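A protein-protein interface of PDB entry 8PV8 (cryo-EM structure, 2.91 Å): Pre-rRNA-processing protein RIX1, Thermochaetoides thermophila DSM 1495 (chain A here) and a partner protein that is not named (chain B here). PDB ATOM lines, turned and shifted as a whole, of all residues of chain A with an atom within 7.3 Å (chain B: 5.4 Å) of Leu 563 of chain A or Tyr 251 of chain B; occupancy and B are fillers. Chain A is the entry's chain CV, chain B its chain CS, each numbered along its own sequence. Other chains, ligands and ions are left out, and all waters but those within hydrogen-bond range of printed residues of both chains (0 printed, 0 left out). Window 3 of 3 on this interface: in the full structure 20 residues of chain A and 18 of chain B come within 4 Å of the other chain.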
ATOM      1  N   PHE A 529      28.432  -0.410 -20.183  1.00  0.00           N
ATOM      2  CA  PHE A 529      28.347   0.472 -19.028  1.00  0.00           C
ATOM      3  C   PHE A 529      29.233   1.697 -19.175  1.00  0.00           C
ATOM      4  O   PHE A 529      28.794   2.816 -18.892  1.00  0.00           O
ATOM      5  CB  PHE A 529      28.746  -0.270 -17.749  1.00  0.00           C
ATOM      6  CG  PHE A 529      28.006  -1.547 -17.523  1.00  0.00           C
ATOM      7  CD1 PHE A 529      26.704  -1.544 -17.061  1.00  0.00           C
ATOM      8  CD2 PHE A 529      28.632  -2.760 -17.747  1.00  0.00           C
ATOM      9  CE1 PHE A 529      26.036  -2.727 -16.847  1.00  0.00           C
ATOM     10  CE2 PHE A 529      27.972  -3.945 -17.532  1.00  0.00           C
ATOM     11  CZ  PHE A 529      26.677  -3.930 -17.078  1.00  0.00           C
ATOM     12  N   THR A 530      30.485   1.506 -19.601  1.00  0.00           N
ATOM     13  CA  THR A 530      31.440   2.610 -19.595  1.00  0.00           C
ATOM     14  C   THR A 530      31.140   3.628 -20.689  1.00  0.00           C
ATOM     15  O   THR A 530      31.174   4.838 -20.442  1.00  0.00           O
ATOM     16  CB  THR A 530      32.866   2.081 -19.746  1.00  0.00           C
ATOM     17  OG1 THR A 530      32.948   1.245 -20.905  1.00  0.00           O
ATOM     18  CG2 THR A 530      33.270   1.284 -18.521  1.00  0.00           C
ATOM     19  N   ARG A 542      19.298  -2.484 -18.386  1.00  0.00           N
ATOM     20  CA  ARG A 542      20.268  -2.375 -17.299  1.00  0.00           C
ATOM     21  C   ARG A 542      20.193  -3.577 -16.365  1.00  0.00           C
ATOM     22  O   ARG A 542      21.227  -4.092 -15.918  1.00  0.00           O
ATOM     23  CB  ARG A 542      20.041  -1.076 -16.524  1.00  0.00           C
ATOM     24  CG  ARG A 542      21.044  -0.815 -15.407  1.00  0.00           C
ATOM     25  CD  ARG A 542      22.481  -0.958 -15.889  1.00  0.00           C
ATOM     26  NE  ARG A 542      23.438  -0.874 -14.793  1.00  0.00           N
ATOM     27  CZ  ARG A 542      24.186   0.188 -14.529  1.00  0.00           C
ATOM     28  NH1 ARG A 542      24.125   1.278 -15.275  1.00  0.00           N
ATOM     29  NH2 ARG A 542      25.018   0.155 -13.493  1.00  0.00           N
ATOM     30  N   ALA A 557      33.013  -5.807 -15.768  1.00  0.00           N
ATOM     31  CA  ALA A 557      31.631  -5.378 -15.942  1.00  0.00           C
ATOM     32  C   ALA A 557      30.988  -5.005 -14.611  1.00  0.00           C
ATOM     33  O   ALA A 557      30.214  -4.045 -14.541  1.00  0.00           O
ATOM     34  CB  ALA A 557      30.828  -6.471 -16.643  1.00  0.00           C
ATOM     35  N   MET A 558      31.297  -5.748 -13.545  1.00  0.00           N
ATOM     36  CA  MET A 558      30.763  -5.410 -12.227  1.00  0.00           C
ATOM     37  C   MET A 558      31.331  -4.087 -11.721  1.00  0.00           C
ATOM     38  O   MET A 558      30.601  -3.263 -11.155  1.00  0.00           O
ATOM     39  CB  MET A 558      31.046  -6.539 -11.234  1.00  0.00           C
ATOM     40  CG  MET A 558      30.406  -7.868 -11.604  1.00  0.00           C
ATOM     41  SD  MET A 558      30.064  -8.919 -10.183  1.00  0.00           S
ATOM     42  CE  MET A 558      31.303 -10.193 -10.398  1.00  0.00           C
ATOM     43  N   LEU A 559      32.634  -3.861 -11.928  1.00  0.00           N
ATOM     44  CA  LEU A 559      33.232  -2.572 -11.588  1.00  0.00           C
ATOM     45  C   LEU A 559      32.625  -1.432 -12.397  1.00  0.00           C
ATOM     46  O   LEU A 559      32.363  -0.356 -11.847  1.00  0.00           O
ATOM     47  CB  LEU A 559      34.751  -2.637 -11.784  1.00  0.00           C
ATOM     48  CG  LEU A 559      35.637  -1.427 -11.470  1.00  0.00           C
ATOM     49  CD1 LEU A 559      36.956  -1.886 -10.916  1.00  0.00           C
ATOM     50  CD2 LEU A 559      35.916  -0.628 -12.734  1.00  0.00           C
ATOM     51  N   ALA A 560      32.397  -1.648 -13.695  1.00  0.00           N
ATOM     52  CA  ALA A 560      31.775  -0.624 -14.523  1.00  0.00           C
ATOM     53  C   ALA A 560      30.343  -0.341 -14.088  1.00  0.00           C
ATOM     54  O   ALA A 560      29.905   0.813 -14.124  1.00  0.00           O
ATOM     55  CB  ALA A 560      31.822  -1.050 -15.988  1.00  0.00           C
ATOM     56  N   SER A 561      29.611  -1.373 -13.665  1.00  0.00           N
ATOM     57  CA  SER A 561      28.270  -1.178 -13.127  1.00  0.00           C
ATOM     58  C   SER A 561      28.302  -0.375 -11.836  1.00  0.00           C
ATOM     59  O   SER A 561      27.437   0.478 -11.605  1.00  0.00           O
ATOM     60  CB  SER A 561      27.606  -2.528 -12.879  1.00  0.00           C
ATOM     61  OG  SER A 561      27.434  -3.248 -14.082  1.00  0.00           O
ATOM     62  N   CYS A 562      29.283  -0.647 -10.973  1.00  0.00           N
ATOM     63  CA  CYS A 562      29.397   0.098  -9.724  1.00  0.00           C
ATOM     64  C   CYS A 562      29.784   1.550  -9.965  1.00  0.00           C
ATOM     65  O   CYS A 562      29.342   2.437  -9.225  1.00  0.00           O
ATOM     66  CB  CYS A 562      30.412  -0.573  -8.801  1.00  0.00           C
ATOM     67  SG  CYS A 562      29.906  -2.193  -8.202  1.00  0.00           S
ATOM     68  N   LEU A 563      30.601   1.816 -10.980  1.00  0.00           N
ATOM     69  CA  LEU A 563      31.080   3.167 -11.242  1.00  0.00           C
ATOM     70  C   LEU A 563      30.198   3.954 -12.202  1.00  0.00           C
ATOM     71  O   LEU A 563      30.397   5.164 -12.346  1.00  0.00           O
ATOM     72  CB  LEU A 563      32.509   3.120 -11.781  1.00  0.00           C
ATOM     73  CG  LEU A 563      33.506   2.507 -10.802  1.00  0.00           C
ATOM     74  CD1 LEU A 563      34.903   2.629 -11.353  1.00  0.00           C
ATOM     75  CD2 LEU A 563      33.383   3.152  -9.431  1.00  0.00           C
ATOM     76  N   HIS A 564      29.232   3.313 -12.856  1.00  0.00           N
ATOM     77  CA  HIS A 564      28.250   4.002 -13.692  1.00  0.00           C
ATOM     78  C   HIS A 564      26.854   3.603 -13.232  1.00  0.00           C
ATOM     79  O   HIS A 564      26.174   2.805 -13.888  1.00  0.00           O
ATOM     80  CB  HIS A 564      28.455   3.667 -15.168  1.00  0.00           C
ATOM     81  CG  HIS A 564      29.793   4.074 -15.698  1.00  0.00           C
ATOM     82  ND1 HIS A 564      30.871   3.217 -15.728  1.00  0.00           N
ATOM     83  CD2 HIS A 564      30.229   5.244 -16.222  1.00  0.00           C
ATOM     84  CE1 HIS A 564      31.913   3.841 -16.246  1.00  0.00           C
ATOM     85  NE2 HIS A 564      31.551   5.073 -16.553  1.00  0.00           N
ATOM     86  N   PRO A 565      26.399   4.137 -12.098  1.00  0.00           N
ATOM     87  CA  PRO A 565      25.104   3.714 -11.555  1.00  0.00           C
ATOM     88  C   PRO A 565      23.945   4.253 -12.380  1.00  0.00           C
ATOM     89  O   PRO A 565      24.048   5.287 -13.043  1.00  0.00           O
ATOM     90  CB  PRO A 565      25.108   4.296 -10.139  1.00  0.00           C
ATOM     91  CG  PRO A 565      26.014   5.470 -10.233  1.00  0.00           C
ATOM     92  CD  PRO A 565      27.058   5.136 -11.238  1.00  0.00           C
ATOM     93  N   ARG A 567      20.320   5.828 -12.730  1.00  0.00           N
ATOM     94  CA  ARG A 567      19.278   6.622 -12.094  1.00  0.00           C
ATOM     95  C   ARG A 567      17.906   6.152 -12.553  1.00  0.00           C
ATOM     96  O   ARG A 567      17.714   5.800 -13.720  1.00  0.00           O
ATOM     97  CB  ARG A 567      19.439   8.107 -12.418  1.00  0.00           C
ATOM     98  CG  ARG A 567      20.665   8.766 -11.829  1.00  0.00           C
ATOM     99  CD  ARG A 567      20.667  10.232 -12.206  1.00  0.00           C
ATOM    100  NE  ARG A 567      21.859  10.936 -11.755  1.00  0.00           N
ATOM    101  CZ  ARG A 567      21.982  11.524 -10.574  1.00  0.00           C
ATOM    102  NH1 ARG A 567      21.012  11.483  -9.676  1.00  0.00           N
ATOM    103  NH2 ARG A 567      23.109  12.166 -10.283  1.00  0.00           N
ATOM    104  N   TYR A 573      19.653   6.652  -7.332  1.00  0.00           N
ATOM    105  CA  TYR A 573      20.498   5.628  -7.918  1.00  0.00           C
ATOM    106  C   TYR A 573      20.014   4.229  -7.544  1.00  0.00           C
ATOM    107  O   TYR A 573      19.474   3.990  -6.460  1.00  0.00           O
ATOM    108  CB  TYR A 573      21.945   5.803  -7.470  1.00  0.00           C
ATOM    109  CG  TYR A 573      22.586   7.124  -7.840  1.00  0.00           C
ATOM    110  CD1 TYR A 573      22.498   8.226  -7.002  1.00  0.00           C
ATOM    111  CD2 TYR A 573      23.287   7.260  -9.027  1.00  0.00           C
ATOM    112  CE1 TYR A 573      23.097   9.420  -7.338  1.00  0.00           C
ATOM    113  CE2 TYR A 573      23.887   8.450  -9.369  1.00  0.00           C
ATOM    114  CZ  TYR A 573      23.795   9.520  -8.513  1.00  0.00           C
ATOM    115  OH  TYR A 573      24.385  10.715  -8.838  1.00  0.00           O
ATOM    116  N   SER A 576      24.100  -0.823  -5.863  1.00  0.00           N
ATOM    117  CA  SER A 576      25.293  -1.204  -6.606  1.00  0.00           C
ATOM    118  C   SER A 576      25.541  -2.706  -6.523  1.00  0.00           C
ATOM    119  O   SER A 576      25.156  -3.364  -5.554  1.00  0.00           O
ATOM    120  CB  SER A 576      26.510  -0.443  -6.082  1.00  0.00           C
ATOM    121  OG  SER A 576      27.688  -0.833  -6.764  1.00  0.00           O
ATOM    122  N   SER A 590      40.409  -4.935  -8.853  1.00  0.00           N
ATOM    123  CA  SER A 590      39.149  -4.223  -9.055  1.00  0.00           C
ATOM    124  C   SER A 590      38.582  -3.692  -7.742  1.00  0.00           C
ATOM    125  O   SER A 590      38.125  -2.546  -7.668  1.00  0.00           O
ATOM    126  CB  SER A 590      38.141  -5.146  -9.739  1.00  0.00           C
ATOM    127  OG  SER A 590      38.679  -5.698 -10.928  1.00  0.00           O
ATOM    128  N   VAL A 593      41.283  -1.224  -5.841  1.00  0.00           N
ATOM    129  CA  VAL A 593      41.130   0.175  -6.219  1.00  0.00           C
ATOM    130  C   VAL A 593      39.986   0.856  -5.471  1.00  0.00           C
ATOM    131  O   VAL A 593      40.173   1.970  -4.960  1.00  0.00           O
ATOM    132  CB  VAL A 593      40.933   0.301  -7.745  1.00  0.00           C
ATOM    133  CG1 VAL A 593      40.432   1.682  -8.125  1.00  0.00           C
ATOM    134  CG2 VAL A 593      42.238   0.013  -8.460  1.00  0.00           C
ATOM    135  N   LEU A 594      38.826   0.209  -5.356  1.00  0.00           N
ATOM    136  CA  LEU A 594      37.693   0.784  -4.641  1.00  0.00           C
ATOM    137  C   LEU A 594      37.922   0.890  -3.140  1.00  0.00           C
ATOM    138  O   LEU A 594      37.191   1.624  -2.469  1.00  0.00           O
ATOM    139  CB  LEU A 594      36.431  -0.037  -4.917  1.00  0.00           C
ATOM    140  CG  LEU A 594      35.750   0.263  -6.254  1.00  0.00           C
ATOM    141  CD1 LEU A 594      34.670  -0.759  -6.552  1.00  0.00           C
ATOM    142  CD2 LEU A 594      35.173   1.666  -6.245  1.00  0.00           C
ATOM    143  N   LYS B 247      21.996  15.806  -5.287  1.00  0.00           N
ATOM    144  CA  LYS B 247      22.565  15.485  -3.988  1.00  0.00           C
ATOM    145  C   LYS B 247      24.079  15.458  -4.104  1.00  0.00           C
ATOM    146  O   LYS B 247      24.611  14.669  -4.902  1.00  0.00           O
ATOM    147  CB  LYS B 247      22.047  14.142  -3.490  1.00  0.00           C
ATOM    148  CG  LYS B 247      22.417  13.827  -2.052  1.00  0.00           C
ATOM    149  CD  LYS B 247      21.657  14.710  -1.079  1.00  0.00           C
ATOM    150  CE  LYS B 247      21.831  14.226   0.351  1.00  0.00           C
ATOM    151  NZ  LYS B 247      23.241  14.353   0.809  1.00  0.00           N
ATOM    152  N   ARG B 249      26.474  14.274  -2.277  1.00  0.00           N
ATOM    153  CA  ARG B 249      27.173  13.087  -1.806  1.00  0.00           C
ATOM    154  C   ARG B 249      26.286  11.849  -1.957  1.00  0.00           C
ATOM    155  O   ARG B 249      26.125  11.040  -1.051  1.00  0.00           O
ATOM    156  CB  ARG B 249      27.646  13.265  -0.363  1.00  0.00           C
ATOM    157  CG  ARG B 249      26.581  13.707   0.627  1.00  0.00           C
ATOM    158  CD  ARG B 249      27.115  13.610   2.043  1.00  0.00           C
ATOM    159  NE  ARG B 249      27.413  12.230   2.403  1.00  0.00           N
ATOM    160  CZ  ARG B 249      28.230  11.870   3.382  1.00  0.00           C
ATOM    161  NH1 ARG B 249      28.849  12.768   4.131  1.00  0.00           N
ATOM    162  NH2 ARG B 249      28.434  10.576   3.615  1.00  0.00           N
ATOM    163  N   ALA B 250      25.689  11.686  -3.134  1.00  0.00           N
ATOM    164  CA  ALA B 250      24.922  10.488  -3.431  1.00  0.00           C
ATOM    165  C   ALA B 250      25.675   9.468  -4.271  1.00  0.00           C
ATOM    166  O   ALA B 250      25.510   8.264  -4.033  1.00  0.00           O
ATOM    167  CB  ALA B 250      23.612  10.851  -4.146  1.00  0.00           C
ATOM    168  N   TYR B 251      26.508   9.912  -5.218  1.00  0.00           N
ATOM    169  CA  TYR B 251      27.220   8.999  -6.108  1.00  0.00           C
ATOM    170  C   TYR B 251      28.192   8.110  -5.340  1.00  0.00           C
ATOM    171  O   TYR B 251      28.271   6.902  -5.591  1.00  0.00           O
ATOM    172  CB  TYR B 251      27.959   9.797  -7.183  1.00  0.00           C
ATOM    173  CG  TYR B 251      28.942   8.987  -8.001  1.00  0.00           C
ATOM    174  CD1 TYR B 251      28.502   8.129  -8.999  1.00  0.00           C
ATOM    175  CD2 TYR B 251      30.310   9.093  -7.786  1.00  0.00           C
ATOM    176  CE1 TYR B 251      29.396   7.393  -9.750  1.00  0.00           C
ATOM    177  CE2 TYR B 251      31.209   8.358  -8.534  1.00  0.00           C
ATOM    178  CZ  TYR B 251      30.745   7.511  -9.514  1.00  0.00           C
ATOM    179  OH  TYR B 251      31.634   6.778 -10.263  1.00  0.00           O
ATOM    180  N   TRP B 252      28.939   8.688  -4.401  1.00  0.00           N
ATOM    181  CA  TRP B 252      29.894   7.899  -3.637  1.00  0.00           C
ATOM    182  C   TRP B 252      29.242   7.140  -2.491  1.00  0.00           C
ATOM    183  O   TRP B 252      29.732   6.069  -2.117  1.00  0.00           O
ATOM    184  CB  TRP B 252      31.012   8.796  -3.106  1.00  0.00           C
ATOM    185  CG  TRP B 252      32.082   9.062  -4.120  1.00  0.00           C
ATOM    186  CD1 TRP B 252      32.405  10.266  -4.670  1.00  0.00           C
ATOM    187  CD2 TRP B 252      32.968   8.101  -4.709  1.00  0.00           C
ATOM    188  NE1 TRP B 252      33.435  10.118  -5.565  1.00  0.00           N
ATOM    189  CE2 TRP B 252      33.801   8.797  -5.606  1.00  0.00           C
ATOM    190  CE3 TRP B 252      33.140   6.721  -4.563  1.00  0.00           C
ATOM    191  CZ2 TRP B 252      34.787   8.162  -6.355  1.00  0.00           C
ATOM    192  CZ3 TRP B 252      34.119   6.092  -5.308  1.00  0.00           C
ATOM    193  CH2 TRP B 252      34.931   6.812  -6.191  1.00  0.00           C
ATOM    194  N   ASP B 253      28.153   7.664  -1.929  1.00  0.00           N
ATOM    195  CA  ASP B 253      27.410   6.935  -0.912  1.00  0.00           C
ATOM    196  C   ASP B 253      26.684   5.722  -1.467  1.00  0.00           C
ATOM    197  O   ASP B 253      26.494   4.748  -0.731  1.00  0.00           O
ATOM    198  CB  ASP B 253      26.412   7.859  -0.214  1.00  0.00           C
ATOM    199  CG  ASP B 253      27.083   8.803   0.758  1.00  0.00           C
ATOM    200  OD1 ASP B 253      28.328   8.898   0.728  1.00  0.00           O
ATOM    201  OD2 ASP B 253      26.368   9.448   1.553  1.00  0.00           O
ATOM    202  N   ASN B 254      26.302   5.746  -2.747  1.00  0.00           N
ATOM    203  CA  ASN B 254      25.769   4.565  -3.416  1.00  0.00           C
ATOM    204  C   ASN B 254      26.763   3.410  -3.462  1.00  0.00           C
ATOM    205  O   ASN B 254      26.342   2.254  -3.574  1.00  0.00           O
ATOM    206  CB  ASN B 254      25.336   4.924  -4.840  1.00  0.00           C
ATOM    207  CG  ASN B 254      24.507   3.836  -5.490  1.00  0.00           C
ATOM    208  OD1 ASN B 254      23.669   3.210  -4.844  1.00  0.00           O
ATOM    209  ND2 ASN B 254      24.744   3.601  -6.775  1.00  0.00           N
ATOM    210  N   ILE B 255      28.061   3.691  -3.363  1.00  0.00           N
ATOM    211  CA  ILE B 255      29.093   2.663  -3.404  1.00  0.00           C
ATOM    212  C   ILE B 255      29.531   2.312  -1.988  1.00  0.00           C
ATOM    213  O   ILE B 255      29.717   1.136  -1.658  1.00  0.00           O
ATOM    214  CB  ILE B 255      30.288   3.129  -4.258  1.00  0.00           C
ATOM    215  CG1 ILE B 255      29.807   3.599  -5.631  1.00  0.00           C
ATOM    216  CG2 ILE B 255      31.311   2.022  -4.407  1.00  0.00           C
ATOM    217  CD1 ILE B 255      30.908   4.127  -6.517  1.00  0.00           C
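Printed residues of chain A that touch a printed residue of chain B: Cys 562, Leu 563, Pro 565, Tyr 573 and Ser 576.
Hydrophobic or aromatic side chains of chain A that line the printed part of chain B: Leu 563, Pro 565 and Tyr 573.
Of the 8 printed residues of chain B, 4 touch a printed residue of chain A.
Printed residues of chain B within 4 Å of Cys 562 of chain A: Ile 255 (3.6 Å).
Printed residues of chain B within 4 Å of Pro 565 of chain A: Tyr 251 and Asn 254.
Printed residues of chain B within 4 Å of Tyr 573 of chain A: Ala 250 and Asn 254.
Printed residues of chain B within 4 Å of Ser 576 of chain A: Asn 254.
Of chain A, only Leu 563 (2.9 Å) and Pro 565 (3.6 Å) come within 4 Å of Tyr 251 of chain B.
The nearest residue of chain B that does not touch Leu 563 of chain A is Trp 252 of chain B (5.1 Å).
The nearest residue of chain A that does not touch Tyr 251 of chain B is Tyr 573 of chain A (4.04 Å).
The nearest printed residue of chain B that does not touch Cys 562 of chain A is Tyr 251 of chain B (5.0 Å).
The backbone carbonyl oxygen (O) of Leu 563 of chain A lies within hydrogen-bond range of the side-chain hydroxyl (OH) of Tyr 251 of chain B (2.9 Å).
Ile 255 of chain B touches Cys 562 of chain A.
Ile 255 of chain B touches Leu 563 of chain A (CD1 to CD2, 3.9 Å).
Tyr 251 of chain B touches Pro 565 of chain A (CE1 to CD, 3.6 Å).
CB of Pro 565 of chain A touches ND2 of Asn 254 of chain B, 3.5 Å away.
Ala 250 of chain B touches Tyr 573 of chain A (CB to CE1, 3.5 Å).
Tyr 573 of chain A touches Asn 254 of chain B.
Ser 576 of chain A touches Asn 254 of chain B.
The side-chain sulfur (SG) of Cys 562 of chain A is in hydrogen-bond range of the backbone carbonyl oxygen (O) of Met 558 of chain A (3.2 Å).
SG of Cys 562 of chain A is in hydrogen-bond range of OG of Ser 576 of chain A (3.0 Å).
The side-chain hydroxyl (OH) of Tyr 573 of chain A is in hydrogen-bond range of the guanidinium group (NH2) of Arg 567 of chain A (2.4 Å).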
